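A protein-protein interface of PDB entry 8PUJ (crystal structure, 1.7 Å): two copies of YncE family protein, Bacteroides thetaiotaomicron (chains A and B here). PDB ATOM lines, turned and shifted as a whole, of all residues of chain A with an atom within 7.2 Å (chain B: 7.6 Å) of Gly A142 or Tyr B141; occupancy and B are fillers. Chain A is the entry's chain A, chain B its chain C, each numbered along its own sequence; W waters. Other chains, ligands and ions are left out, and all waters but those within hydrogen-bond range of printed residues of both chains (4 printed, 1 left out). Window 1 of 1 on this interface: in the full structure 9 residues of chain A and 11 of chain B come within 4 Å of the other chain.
OH of Tyr A141 sits at hydrogen-bond distance from N of Lys B143, at 3.1 Å. The backbone NH (N) of Lys A143 lies within hydrogen-bond range of the side-chain hydroxyl (OH) of Tyr B141 (3.2 Å). The side-chain carboxylate (OD1) of Asp B211 lies within salt-bridge range of the side-chain amino group (NZ) of Lys A143 (3.9 Å). OE1 of Glu B213 is in salt-bridge range of NZ of Lys A143 (3.6 Å). The side-chain hydroxyl (OH) of Tyr A144 lies within hydrogen-bond range of the side-chain carboxylate (OE1) of Glu B213 (2.7 Å). The side-chain carboxylate (OE1) of Glu A213 is in salt-bridge range of the side-chain amino group (NZ) of Lys B143 (3.0 Å). OE1 of Glu A213 sits at hydrogen-bond distance from OH of Tyr B144 (2.8 Å).
The side-chain amide nitrogen (NE2) of Gln A140 lies within hydrogen-bond range of the backbone carbonyl oxygen (O) of Gly A142 (3.0 Å). NE2 of Gln B140 lies within hydrogen-bond range of O of Gly B142 (3.0 Å). O of Lys B143 lies within hydrogen-bond range of OG1 of Thr B161 (2.7 Å). O of Phe B185 is in hydrogen-bond range of N of Ala B212 (3.1 Å). The side-chain carboxylate of Asp B211 sits close to the backbone NH of Glu B213 (3.5 Å). OD2 of Asp B211 sits at hydrogen-bond distance from OG1 of Thr B214 (2.7 Å).
Gly B142 touches Tyr A141. Tyr A141 touches Tyr B144. Tyr B141 touches Gly A142. Gly A142 touches Phe B185. Phe B185 touches Lys A143 (CD1 to CB, 3.3 Å). OH of Tyr B141 touches CE2 of Tyr A144, at 3.9 Å. OG1 of Thr A161 touches CE1 of Phe B185, 3.9 Å away. Gly B142 touches Phe A185 (O to CZ, 3.8 Å). Lys B143 touches Phe A185 (CB to CD1, 3.4 Å). Thr B161 touches Phe A185.
Of the printed residues of chain A, Asp B211 touches Lys A143. Of the printed residues of chain A, Lys B143 touches Tyr A141, Phe A185 and Glu A213. Of the printed residues of chain A, Gly B142 touches Tyr A141 (3.5 Å) and Phe A185 (3.8 Å). Of the printed residues of chain A, Glu B213 touches Lys A143 (3.3 Å) and Tyr A144 (2.7 Å). Printed residues of chain A within 4 Å of Tyr B144: Tyr A141 (3.9 Å) and Glu A213 (2.8 Å). Val A145 touches none of the printed residues of chain B. The nearest residue of chain A that does not touch Tyr B141 is Tyr A141 (4.2 Å).
Of the 21 printed residues of chain B, 8 touch a printed residue of chain A. Printed residues of chain B that touch a printed residue of chain A: Tyr B141, Gly B142, Lys B143, Tyr B144, Thr B161, Phe B185, Asp B211 and Glu B213. Of the 11 printed residues of chain A, 7 touch a printed residue of chain B. Among the printed residues, 17 pairs touch across the chains. Among the printed residues, Asp or Glu carboxylates within 4 Å of a Lys or Arg side-chain nitrogen of the other chain: Lys A143 with Asp B211 (3.9 Å), Lys A143 with Glu B213 (3.6 Å) and Glu A213 with Lys B143 (3.0 Å).
Tyr A141 touches Tyr B144, and with the chains exchanged Tyr A144 touches Tyr B141. Lys A143 touches Phe B185, and with the chains exchanged Phe A185 touches Lys B143. Tyr A144 touches Glu B213, and with the chains exchanged Glu A213 touches Tyr B144. Thr A161 touches Phe B185, and with the chains exchanged Phe A185 touches Thr B161. Positions printed for both chains: 140, 141, 142, 143, 144, 145, 146, 161, 181, 185 and 213.
Water W4 lies within hydrogen-bond range of the backbone carbonyl oxygen (O) of Asn B184 (2.7 Å), the side-chain amino group (NZ) of Lys A143 (2.7 Å) and the side-chain amino group (NZ) of Lys B186 (3.2 Å). Water W1 lies within hydrogen-bond range of OE1 of Glu A213 and NZ of Lys B143. Water W2 lies within hydrogen-bond range of the side-chain carboxylate (OD2) of Asp B211, the side-chain carboxylate (OE1) of Glu B213 and the side-chain amino group (NZ) of Lys A143. Water W3 lies within hydrogen-bond range of the backbone carbonyl oxygen of Phe A185 (2.8 Å), the backbone NH of Glu A213 (2.9 Å) and the side-chain amino group of Lys B143 (3.2 Å).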
ATOM      1  N   GLN A 140       2.647  16.967 -24.207  1.00  0.00           N
ATOM      2  CA  GLN A 140       1.515  16.094 -23.905  1.00  0.00           C
ATOM      3  C   GLN A 140       1.179  15.295 -25.153  1.00  0.00           C
ATOM      4  O   GLN A 140       1.153  15.843 -26.258  1.00  0.00           O
ATOM      5  CB  GLN A 140       0.308  16.916 -23.453  1.00  0.00           C
ATOM      6  CG  GLN A 140      -0.874  15.980 -23.025  1.00  0.00           C
ATOM      7  CD  GLN A 140      -1.889  16.683 -22.144  1.00  0.00           C
ATOM      8  OE1 GLN A 140      -1.652  17.805 -21.680  1.00  0.00           O
ATOM      9  NE2 GLN A 140      -3.043  16.034 -21.926  1.00  0.00           N
ATOM     10  N   TYR A 141       0.912  13.995 -24.964  1.00  0.00           N
ATOM     11  CA  TYR A 141       0.461  13.117 -26.042  1.00  0.00           C
ATOM     12  C   TYR A 141      -0.756  12.387 -25.478  1.00  0.00           C
ATOM     13  O   TYR A 141      -0.618  11.618 -24.526  1.00  0.00           O
ATOM     14  CB  TYR A 141       1.539  12.112 -26.444  1.00  0.00           C
ATOM     15  CG  TYR A 141       0.970  11.195 -27.538  1.00  0.00           C
ATOM     16  CD1 TYR A 141       0.954  11.605 -28.847  1.00  0.00           C
ATOM     17  CD2 TYR A 141       0.318   9.977 -27.194  1.00  0.00           C
ATOM     18  CE1 TYR A 141       0.371  10.797 -29.861  1.00  0.00           C
ATOM     19  CE2 TYR A 141      -0.251   9.169 -28.180  1.00  0.00           C
ATOM     20  CZ  TYR A 141      -0.238   9.612 -29.502  1.00  0.00           C
ATOM     21  OH  TYR A 141      -0.852   8.842 -30.480  1.00  0.00           O
ATOM     22  N   GLY A 142      -1.932  12.660 -26.012  1.00  0.00           N
ATOM     23  CA  GLY A 142      -3.104  12.003 -25.462  1.00  0.00           C
ATOM     24  C   GLY A 142      -3.289  12.332 -23.978  1.00  0.00           C
ATOM     25  O   GLY A 142      -3.282  13.505 -23.571  1.00  0.00           O
ATOM     26  N   LYS A 143      -3.460  11.297 -23.156  1.00  0.00           N
ATOM     27  CA  LYS A 143      -3.643  11.486 -21.732  1.00  0.00           C
ATOM     28  C   LYS A 143      -2.329  11.649 -20.980  1.00  0.00           C
ATOM     29  O   LYS A 143      -2.337  11.893 -19.767  1.00  0.00           O
ATOM     30  CB  LYS A 143      -4.462  10.317 -21.166  1.00  0.00           C
ATOM     31  CG  LYS A 143      -3.672   9.042 -21.047  1.00  0.00           C
ATOM     32  CD  LYS A 143      -4.548   8.007 -20.271  1.00  0.00           C
ATOM     33  CE  LYS A 143      -4.989   6.883 -21.164  1.00  0.00           C
ATOM     34  NZ  LYS A 143      -5.674   5.795 -20.334  1.00  0.00           N
ATOM     35  N   TYR A 144      -1.186  11.559 -21.664  1.00  0.00           N
ATOM     36  CA  TYR A 144       0.078  11.504 -20.950  1.00  0.00           C
ATOM     37  C   TYR A 144       0.843  12.807 -21.088  1.00  0.00           C
ATOM     38  O   TYR A 144       0.907  13.377 -22.174  1.00  0.00           O
ATOM     39  CB  TYR A 144       0.958  10.359 -21.461  1.00  0.00           C
ATOM     40  CG  TYR A 144       0.307   9.020 -21.192  1.00  0.00           C
ATOM     41  CD1 TYR A 144       0.188   8.537 -19.888  1.00  0.00           C
ATOM     42  CD2 TYR A 144      -0.230   8.294 -22.262  1.00  0.00           C
ATOM     43  CE1 TYR A 144      -0.449   7.305 -19.641  1.00  0.00           C
ATOM     44  CE2 TYR A 144      -0.874   7.078 -22.038  1.00  0.00           C
ATOM     45  CZ  TYR A 144      -0.949   6.587 -20.727  1.00  0.00           C
ATOM     46  OH  TYR A 144      -1.575   5.381 -20.526  1.00  0.00           O
ATOM     47  N   VAL A 145       1.491  13.218 -19.996  1.00  0.00           N
ATOM     48  CA  VAL A 145       2.504  14.271 -20.064  1.00  0.00           C
ATOM     49  C   VAL A 145       3.859  13.600 -19.932  1.00  0.00           C
ATOM     50  O   VAL A 145       4.093  12.817 -18.997  1.00  0.00           O
ATOM     51  CB  VAL A 145       2.306  15.317 -18.969  1.00  0.00           C
ATOM     52  CG1 VAL A 145       3.559  16.261 -18.929  1.00  0.00           C
ATOM     53  CG2 VAL A 145       1.102  16.179 -19.328  1.00  0.00           C
ATOM     54  N   TYR A 146       4.759  13.935 -20.844  1.00  0.00           N
ATOM     55  CA  TYR A 146       6.136  13.484 -20.734  1.00  0.00           C
ATOM     56  C   TYR A 146       6.976  14.676 -20.283  1.00  0.00           C
ATOM     57  O   TYR A 146       6.707  15.837 -20.670  1.00  0.00           O
ATOM     58  CB  TYR A 146       6.625  13.001 -22.075  1.00  0.00           C
ATOM     59  CG  TYR A 146       6.003  11.735 -22.565  1.00  0.00           C
ATOM     60  CD1 TYR A 146       6.441  10.546 -22.078  1.00  0.00           C
ATOM     61  CD2 TYR A 146       5.052  11.753 -23.584  1.00  0.00           C
ATOM     62  CE1 TYR A 146       5.938   9.337 -22.536  1.00  0.00           C
ATOM     63  CE2 TYR A 146       4.530  10.539 -24.081  1.00  0.00           C
ATOM     64  CZ  TYR A 146       4.982   9.357 -23.534  1.00  0.00           C
ATOM     65  OH  TYR A 146       4.530   8.139 -24.001  1.00  0.00           O
ATOM     66  N   THR A 161      -2.239  11.867 -16.854  1.00  0.00           N
ATOM     67  CA  THR A 161      -2.927  13.036 -16.318  1.00  0.00           C
ATOM     68  C   THR A 161      -4.261  12.692 -15.719  1.00  0.00           C
ATOM     69  O   THR A 161      -4.827  13.552 -15.041  1.00  0.00           O
ATOM     70  CB  THR A 161      -3.159  14.117 -17.396  1.00  0.00           C
ATOM     71  OG1 THR A 161      -4.013  13.595 -18.449  1.00  0.00           O
ATOM     72  CG2 THR A 161      -1.882  14.564 -18.009  1.00  0.00           C
ATOM     73  N   MET A 181       7.752  18.108 -29.273  1.00  0.00           N
ATOM     74  CA  MET A 181       7.056  17.047 -30.025  1.00  0.00           C
ATOM     75  C   MET A 181       6.757  17.523 -31.453  1.00  0.00           C
ATOM     76  O   MET A 181       6.164  18.588 -31.605  1.00  0.00           O
ATOM     77  CB  MET A 181       5.741  16.623 -29.383  1.00  0.00           C
ATOM     78  CG  MET A 181       5.203  15.437 -30.139  1.00  0.00           C
ATOM     79  SD  MET A 181       4.171  14.375 -29.132  1.00  0.00           S
ATOM     80  CE  MET A 181       2.791  15.517 -29.000  1.00  0.00           C
ATOM     81  N   PHE A 185       4.369  13.292 -34.173  1.00  0.00           N
ATOM     82  CA  PHE A 185       4.221  12.863 -32.781  1.00  0.00           C
ATOM     83  C   PHE A 185       5.419  12.049 -32.319  1.00  0.00           C
ATOM     84  O   PHE A 185       5.278  11.049 -31.598  1.00  0.00           O
ATOM     85  CB  PHE A 185       2.920  12.108 -32.574  1.00  0.00           C
ATOM     86  CG  PHE A 185       1.721  12.944 -32.923  1.00  0.00           C
ATOM     87  CD1 PHE A 185       1.279  13.030 -34.249  1.00  0.00           C
ATOM     88  CD2 PHE A 185       1.075  13.650 -31.955  1.00  0.00           C
ATOM     89  CE1 PHE A 185       0.149  13.812 -34.574  1.00  0.00           C
ATOM     90  CE2 PHE A 185      -0.051  14.446 -32.259  1.00  0.00           C
ATOM     91  CZ  PHE A 185      -0.503  14.514 -33.563  1.00  0.00           C
ATOM     92  N   GLU A 213       3.715   7.734 -28.948  1.00  0.00           N
ATOM     93  CA  GLU A 213       2.661   6.756 -28.687  1.00  0.00           C
ATOM     94  C   GLU A 213       3.192   5.579 -27.873  1.00  0.00           C
ATOM     95  O   GLU A 213       2.575   5.179 -26.869  1.00  0.00           O
ATOM     96  CB  GLU A 213       2.054   6.301 -30.028  1.00  0.00           C
ATOM     97  CG  GLU A 213       0.985   5.198 -29.889  1.00  0.00           C
ATOM     98  CD  GLU A 213       0.595   4.643 -31.259  1.00  0.00           C
ATOM     99  OE1 GLU A 213       0.961   5.253 -32.278  1.00  0.00           O
ATOM    100  OE2 GLU A 213      -0.059   3.582 -31.314  1.00  0.00           O
ATOM    101  N   HIS B  92     -13.630  18.495 -38.502  1.00  0.00           N
ATOM    102  CA  HIS B  92     -12.720  18.419 -37.368  1.00  0.00           C
ATOM    103  C   HIS B  92     -11.347  18.852 -37.835  1.00  0.00           C
ATOM    104  O   HIS B  92     -10.832  18.334 -38.855  1.00  0.00           O
ATOM    105  CB  HIS B  92     -12.631  16.985 -36.837  1.00  0.00           C
ATOM    106  CG  HIS B  92     -11.544  16.795 -35.832  1.00  0.00           C
ATOM    107  ND1 HIS B  92     -11.684  17.199 -34.518  1.00  0.00           N
ATOM    108  CD2 HIS B  92     -10.305  16.260 -35.937  1.00  0.00           C
ATOM    109  CE1 HIS B  92     -10.569  16.928 -33.852  1.00  0.00           C
ATOM    110  NE2 HIS B  92      -9.714  16.368 -34.689  1.00  0.00           N
ATOM    111  N   VAL B 139     -13.518  12.377 -32.927  1.00  0.00           N
ATOM    112  CA  VAL B 139     -12.782  12.840 -31.767  1.00  0.00           C
ATOM    113  C   VAL B 139     -11.326  12.517 -32.042  1.00  0.00           C
ATOM    114  O   VAL B 139     -11.022  11.666 -32.870  1.00  0.00           O
ATOM    115  CB  VAL B 139     -13.237  12.163 -30.455  1.00  0.00           C
ATOM    116  CG1 VAL B 139     -14.670  12.509 -30.128  1.00  0.00           C
ATOM    117  CG2 VAL B 139     -13.077  10.681 -30.520  1.00  0.00           C
ATOM    118  N   GLN B 140     -10.424  13.196 -31.355  1.00  0.00           N
ATOM    119  CA  GLN B 140      -9.008  12.969 -31.623  1.00  0.00           C
ATOM    120  C   GLN B 140      -8.319  12.568 -30.328  1.00  0.00           C
ATOM    121  O   GLN B 140      -8.553  13.187 -29.284  1.00  0.00           O
ATOM    122  CB  GLN B 140      -8.366  14.220 -32.211  1.00  0.00           C
ATOM    123  CG  GLN B 140      -6.894  13.948 -32.576  1.00  0.00           C
ATOM    124  CD  GLN B 140      -6.292  14.965 -33.523  1.00  0.00           C
ATOM    125  OE1 GLN B 140      -6.995  15.755 -34.157  1.00  0.00           O
ATOM    126  NE2 GLN B 140      -4.978  14.905 -33.675  1.00  0.00           N
ATOM    127  N   TYR B 141      -7.485  11.523 -30.388  1.00  0.00           N
ATOM    128  CA  TYR B 141      -6.674  11.104 -29.250  1.00  0.00           C
ATOM    129  C   TYR B 141      -5.250  11.004 -29.764  1.00  0.00           C
ATOM    130  O   TYR B 141      -4.991  10.196 -30.646  1.00  0.00           O
ATOM    131  CB  TYR B 141      -7.135   9.737 -28.691  1.00  0.00           C
ATOM    132  CG  TYR B 141      -6.198   9.314 -27.572  1.00  0.00           C
ATOM    133  CD1 TYR B 141      -6.458   9.715 -26.259  1.00  0.00           C
ATOM    134  CD2 TYR B 141      -5.029   8.584 -27.844  1.00  0.00           C
ATOM    135  CE1 TYR B 141      -5.575   9.383 -25.220  1.00  0.00           C
ATOM    136  CE2 TYR B 141      -4.101   8.273 -26.818  1.00  0.00           C
ATOM    137  CZ  TYR B 141      -4.412   8.671 -25.518  1.00  0.00           C
ATOM    138  OH  TYR B 141      -3.525   8.420 -24.489  1.00  0.00           O
ATOM    139  N   GLY B 142      -4.355  11.857 -29.281  1.00  0.00           N
ATOM    140  CA  GLY B 142      -2.988  11.795 -29.839  1.00  0.00           C
ATOM    141  C   GLY B 142      -2.987  12.007 -31.350  1.00  0.00           C
ATOM    142  O   GLY B 142      -3.508  12.998 -31.879  1.00  0.00           O
ATOM    143  N   LYS B 143      -2.333  11.082 -32.056  1.00  0.00           N
ATOM    144  CA  LYS B 143      -2.228  11.199 -33.503  1.00  0.00           C
ATOM    145  C   LYS B 143      -3.447  10.647 -34.218  1.00  0.00           C
ATOM    146  O   LYS B 143      -3.490  10.681 -35.461  1.00  0.00           O
ATOM    147  CB  LYS B 143      -0.958  10.502 -33.978  1.00  0.00           C
ATOM    148  CG  LYS B 143      -1.041   8.994 -34.062  1.00  0.00           C
ATOM    149  CD  LYS B 143       0.292   8.453 -34.655  1.00  0.00           C
ATOM    150  CE  LYS B 143       1.276   8.059 -33.595  1.00  0.00           C
ATOM    151  NZ  LYS B 143       2.336   7.148 -34.177  1.00  0.00           N
ATOM    152  N   TYR B 144      -4.398  10.060 -33.483  1.00  0.00           N
ATOM    153  CA  TYR B 144      -5.497   9.359 -34.140  1.00  0.00           C
ATOM    154  C   TYR B 144      -6.798  10.131 -34.068  1.00  0.00           C
ATOM    155  O   TYR B 144      -7.162  10.666 -33.021  1.00  0.00           O
ATOM    156  CB  TYR B 144      -5.709   7.993 -33.538  1.00  0.00           C
ATOM    157  CG  TYR B 144      -4.478   7.125 -33.691  1.00  0.00           C
ATOM    158  CD1 TYR B 144      -4.160   6.578 -34.913  1.00  0.00           C
ATOM    159  CD2 TYR B 144      -3.669   6.877 -32.584  1.00  0.00           C
ATOM    160  CE1 TYR B 144      -2.986   5.762 -35.062  1.00  0.00           C
ATOM    161  CE2 TYR B 144      -2.513   6.071 -32.713  1.00  0.00           C
ATOM    162  CZ  TYR B 144      -2.212   5.531 -33.939  1.00  0.00           C
ATOM    163  OH  TYR B 144      -1.096   4.722 -34.104  1.00  0.00           O
ATOM    164  N   VAL B 145      -7.548  10.083 -35.159  1.00  0.00           N
ATOM    165  CA  VAL B 145      -8.941  10.530 -35.174  1.00  0.00           C
ATOM    166  C   VAL B 145      -9.816   9.287 -35.199  1.00  0.00           C
ATOM    167  O   VAL B 145      -9.634   8.398 -36.047  1.00  0.00           O
ATOM    168  CB  VAL B 145      -9.206  11.445 -36.388  1.00  0.00           C
ATOM    169  CG1 VAL B 145     -10.735  11.617 -36.631  1.00  0.00           C
ATOM    170  CG2 VAL B 145      -8.583  12.804 -36.133  1.00  0.00           C
ATOM    171  N   TYR B 146     -10.800   9.248 -34.313  1.00  0.00           N
ATOM    172  CA  TYR B 146     -11.821   8.216 -34.303  1.00  0.00           C
ATOM    173  C   TYR B 146     -13.108   8.807 -34.861  1.00  0.00           C
ATOM    174  O   TYR B 146     -13.394   9.993 -34.653  1.00  0.00           O
ATOM    175  CB  TYR B 146     -12.054   7.713 -32.888  1.00  0.00           C
ATOM    176  CG  TYR B 146     -10.875   6.931 -32.325  1.00  0.00           C
ATOM    177  CD1 TYR B 146     -10.683   5.613 -32.695  1.00  0.00           C
ATOM    178  CD2 TYR B 146     -10.004   7.515 -31.447  1.00  0.00           C
ATOM    179  CE1 TYR B 146      -9.608   4.875 -32.166  1.00  0.00           C
ATOM    180  CE2 TYR B 146      -8.919   6.782 -30.906  1.00  0.00           C
ATOM    181  CZ  TYR B 146      -8.753   5.489 -31.292  1.00  0.00           C
ATOM    182  OH  TYR B 146      -7.709   4.751 -30.745  1.00  0.00           O
ATOM    183  N   LYS B 158     -10.542   4.182 -36.973  1.00  0.00           N
ATOM    184  CA  LYS B 158      -9.382   4.839 -36.368  1.00  0.00           C
ATOM    185  C   LYS B 158      -8.503   5.316 -37.516  1.00  0.00           C
ATOM    186  O   LYS B 158      -8.059   4.500 -38.339  1.00  0.00           O
ATOM    187  CB  LYS B 158      -8.624   3.843 -35.480  1.00  0.00           C
ATOM    188  CG  LYS B 158      -7.356   4.435 -34.807  1.00  0.00           C
ATOM    189  CD  LYS B 158      -6.744   3.335 -33.938  1.00  0.00           C
ATOM    190  CE  LYS B 158      -5.530   3.841 -33.150  1.00  0.00           C
ATOM    191  NZ  LYS B 158      -4.844   2.598 -32.552  1.00  0.00           N
ATOM    192  N   ILE B 159      -8.223   6.611 -37.558  1.00  0.00           N
ATOM    193  CA  ILE B 159      -7.460   7.224 -38.654  1.00  0.00           C
ATOM    194  C   ILE B 159      -6.147   7.755 -38.095  1.00  0.00           C
ATOM    195  O   ILE B 159      -6.144   8.517 -37.120  1.00  0.00           O
ATOM    196  CB  ILE B 159      -8.260   8.379 -39.288  1.00  0.00           C
ATOM    197  CG1 ILE B 159      -9.519   7.845 -39.978  1.00  0.00           C
ATOM    198  CG2 ILE B 159      -7.411   9.237 -40.266  1.00  0.00           C
ATOM    199  CD1 ILE B 159     -10.551   8.988 -40.235  1.00  0.00           C
ATOM    200  N   THR B 161      -3.559  10.418 -38.289  1.00  0.00           N
ATOM    201  CA  THR B 161      -3.509  11.715 -38.962  1.00  0.00           C
ATOM    202  C   THR B 161      -2.147  11.989 -39.570  1.00  0.00           C
ATOM    203  O   THR B 161      -2.043  12.909 -40.370  1.00  0.00           O
ATOM    204  CB  THR B 161      -3.847  12.856 -38.014  1.00  0.00           C
ATOM    205  OG1 THR B 161      -2.865  12.875 -36.968  1.00  0.00           O
ATOM    206  CG2 THR B 161      -5.189  12.608 -37.395  1.00  0.00           C
ATOM    207  N   MET B 181     -15.555  12.229 -26.299  1.00  0.00           N
ATOM    208  CA  MET B 181     -14.465  11.713 -25.437  1.00  0.00           C
ATOM    209  C   MET B 181     -14.470  12.447 -24.085  1.00  0.00           C
ATOM    210  O   MET B 181     -14.423  13.662 -24.073  1.00  0.00           O
ATOM    211  CB  MET B 181     -13.078  11.900 -26.042  1.00  0.00           C
ATOM    212  CG  MET B 181     -12.060  11.095 -25.273  1.00  0.00           C
ATOM    213  SD  MET B 181     -10.568  10.771 -26.217  1.00  0.00           S
ATOM    214  CE  MET B 181      -9.985  12.448 -26.487  1.00  0.00           C
ATOM    215  N   ASN B 184     -11.572  11.286 -18.846  1.00  0.00           N
ATOM    216  CA  ASN B 184     -10.712  10.128 -18.624  1.00  0.00           C
ATOM    217  C   ASN B 184     -10.186   9.547 -19.940  1.00  0.00           C
ATOM    218  O   ASN B 184      -9.592   8.450 -19.937  1.00  0.00           O
ATOM    219  CB  ASN B 184     -11.477   9.063 -17.854  1.00  0.00           C
ATOM    220  CG  ASN B 184     -11.826   9.531 -16.477  1.00  0.00           C
ATOM    221  OD1 ASN B 184     -10.995  10.192 -15.832  1.00  0.00           O
ATOM    222  ND2 ASN B 184     -13.022   9.224 -16.018  1.00  0.00           N
ATOM    223  N   PHE B 185     -10.408  10.256 -21.064  1.00  0.00           N
ATOM    224  CA  PHE B 185     -10.028   9.802 -22.391  1.00  0.00           C
ATOM    225  C   PHE B 185     -10.677   8.469 -22.710  1.00  0.00           C
ATOM    226  O   PHE B 185     -10.060   7.588 -23.332  1.00  0.00           O
ATOM    227  CB  PHE B 185      -8.511   9.740 -22.555  1.00  0.00           C
ATOM    228  CG  PHE B 185      -7.861  11.092 -22.384  1.00  0.00           C
ATOM    229  CD1 PHE B 185      -7.548  11.545 -21.095  1.00  0.00           C
ATOM    230  CD2 PHE B 185      -7.623  11.892 -23.463  1.00  0.00           C
ATOM    231  CE1 PHE B 185      -6.932  12.797 -20.921  1.00  0.00           C
ATOM    232  CE2 PHE B 185      -7.032  13.182 -23.296  1.00  0.00           C
ATOM    233  CZ  PHE B 185      -6.709  13.611 -22.004  1.00  0.00           C
ATOM    234  N   LYS B 186     -11.936   8.338 -22.287  1.00  0.00           N
ATOM    235  CA  LYS B 186     -12.802   7.269 -22.737  1.00  0.00           C
ATOM    236  C   LYS B 186     -13.773   7.853 -23.755  1.00  0.00           C
ATOM    237  O   LYS B 186     -14.395   8.911 -23.509  1.00  0.00           O
ATOM    238  CB  LYS B 186     -13.606   6.655 -21.605  1.00  0.00           C
ATOM    239  CG  LYS B 186     -12.795   6.250 -20.346  1.00  0.00           C
ATOM    240  CD  LYS B 186     -11.665   5.277 -20.709  1.00  0.00           C
ATOM    241  CE  LYS B 186     -11.043   4.818 -19.351  1.00  0.00           C
ATOM    242  NZ  LYS B 186      -9.906   3.906 -19.577  1.00  0.00           N
ATOM    243  N   MET B 187     -13.914   7.148 -24.871  1.00  0.00           N
ATOM    244  CA  MET B 187     -14.869   7.537 -25.904  1.00  0.00           C
ATOM    245  C   MET B 187     -16.219   6.923 -25.571  1.00  0.00           C
ATOM    246  O   MET B 187     -16.311   5.800 -25.095  1.00  0.00           O
ATOM    247  CB  MET B 187     -14.430   7.043 -27.282  1.00  0.00           C
ATOM    248  CG  MET B 187     -13.153   7.677 -27.723  1.00  0.00           C
ATOM    249  SD  MET B 187     -12.781   7.205 -29.422  1.00  0.00           S
ATOM    250  CE  MET B 187     -12.240   5.491 -29.251  1.00  0.00           C
ATOM    251  N   ASP B 211     -12.040   2.686 -24.410  1.00  0.00           N
ATOM    252  CA  ASP B 211     -10.789   3.381 -24.070  1.00  0.00           C
ATOM    253  C   ASP B 211     -10.154   3.976 -25.336  1.00  0.00           C
ATOM    254  O   ASP B 211      -9.958   3.293 -26.341  1.00  0.00           O
ATOM    255  CB  ASP B 211      -9.811   2.389 -23.416  1.00  0.00           C
ATOM    256  CG  ASP B 211      -8.541   3.054 -22.955  1.00  0.00           C
ATOM    257  OD1 ASP B 211      -8.663   4.041 -22.213  1.00  0.00           O
ATOM    258  OD2 ASP B 211      -7.420   2.667 -23.389  1.00  0.00           O
ATOM    259  N   ALA B 212      -9.829   5.266 -25.313  1.00  0.00           N
ATOM    260  CA  ALA B 212      -9.289   5.867 -26.518  1.00  0.00           C
ATOM    261  C   ALA B 212      -7.852   5.436 -26.761  1.00  0.00           C
ATOM    262  O   ALA B 212      -7.451   5.281 -27.904  1.00  0.00           O
ATOM    263  CB  ALA B 212      -9.274   7.397 -26.429  1.00  0.00           C
ATOM    264  N   GLU B 213      -7.056   5.248 -25.715  1.00  0.00           N
ATOM    265  CA  GLU B 213      -5.660   4.903 -25.969  1.00  0.00           C
ATOM    266  C   GLU B 213      -5.547   3.542 -26.629  1.00  0.00           C
ATOM    267  O   GLU B 213      -4.763   3.363 -27.569  1.00  0.00           O
ATOM    268  CB  GLU B 213      -4.874   4.930 -24.673  1.00  0.00           C
ATOM    269  CG  GLU B 213      -3.407   4.515 -24.946  1.00  0.00           C
ATOM    270  CD  GLU B 213      -2.607   4.327 -23.670  1.00  0.00           C
ATOM    271  OE1 GLU B 213      -3.171   4.478 -22.564  1.00  0.00           O
ATOM    272  OE2 GLU B 213      -1.401   3.986 -23.784  1.00  0.00           O
ATOM    273  N   THR B 214      -6.332   2.577 -26.163  1.00  0.00           N
ATOM    274  CA  THR B 214      -6.202   1.209 -26.645  1.00  0.00           C
ATOM    275  C   THR B 214      -7.316   0.782 -27.574  1.00  0.00           C
ATOM    276  O   THR B 214      -7.252  -0.344 -28.077  1.00  0.00           O
ATOM    277  CB  THR B 214      -6.141   0.246 -25.465  1.00  0.00           C
ATOM    278  OG1 THR B 214      -7.404   0.285 -24.756  1.00  0.00           O
ATOM    279  CG2 THR B 214      -4.968   0.690 -24.546  1.00  0.00           C
HETATM  280  O   HOH W   1       3.625   4.857 -32.940  1.00  0.00           O
HETATM  281  O   HOH W   2      -5.453   3.092 -21.432  1.00  0.00           O
HETATM  282  O   HOH W   3       3.779   8.674 -31.710  1.00  0.00           O
HETATM  283  O   HOH W   4      -7.998   6.472 -19.175  1.00  0.00           O
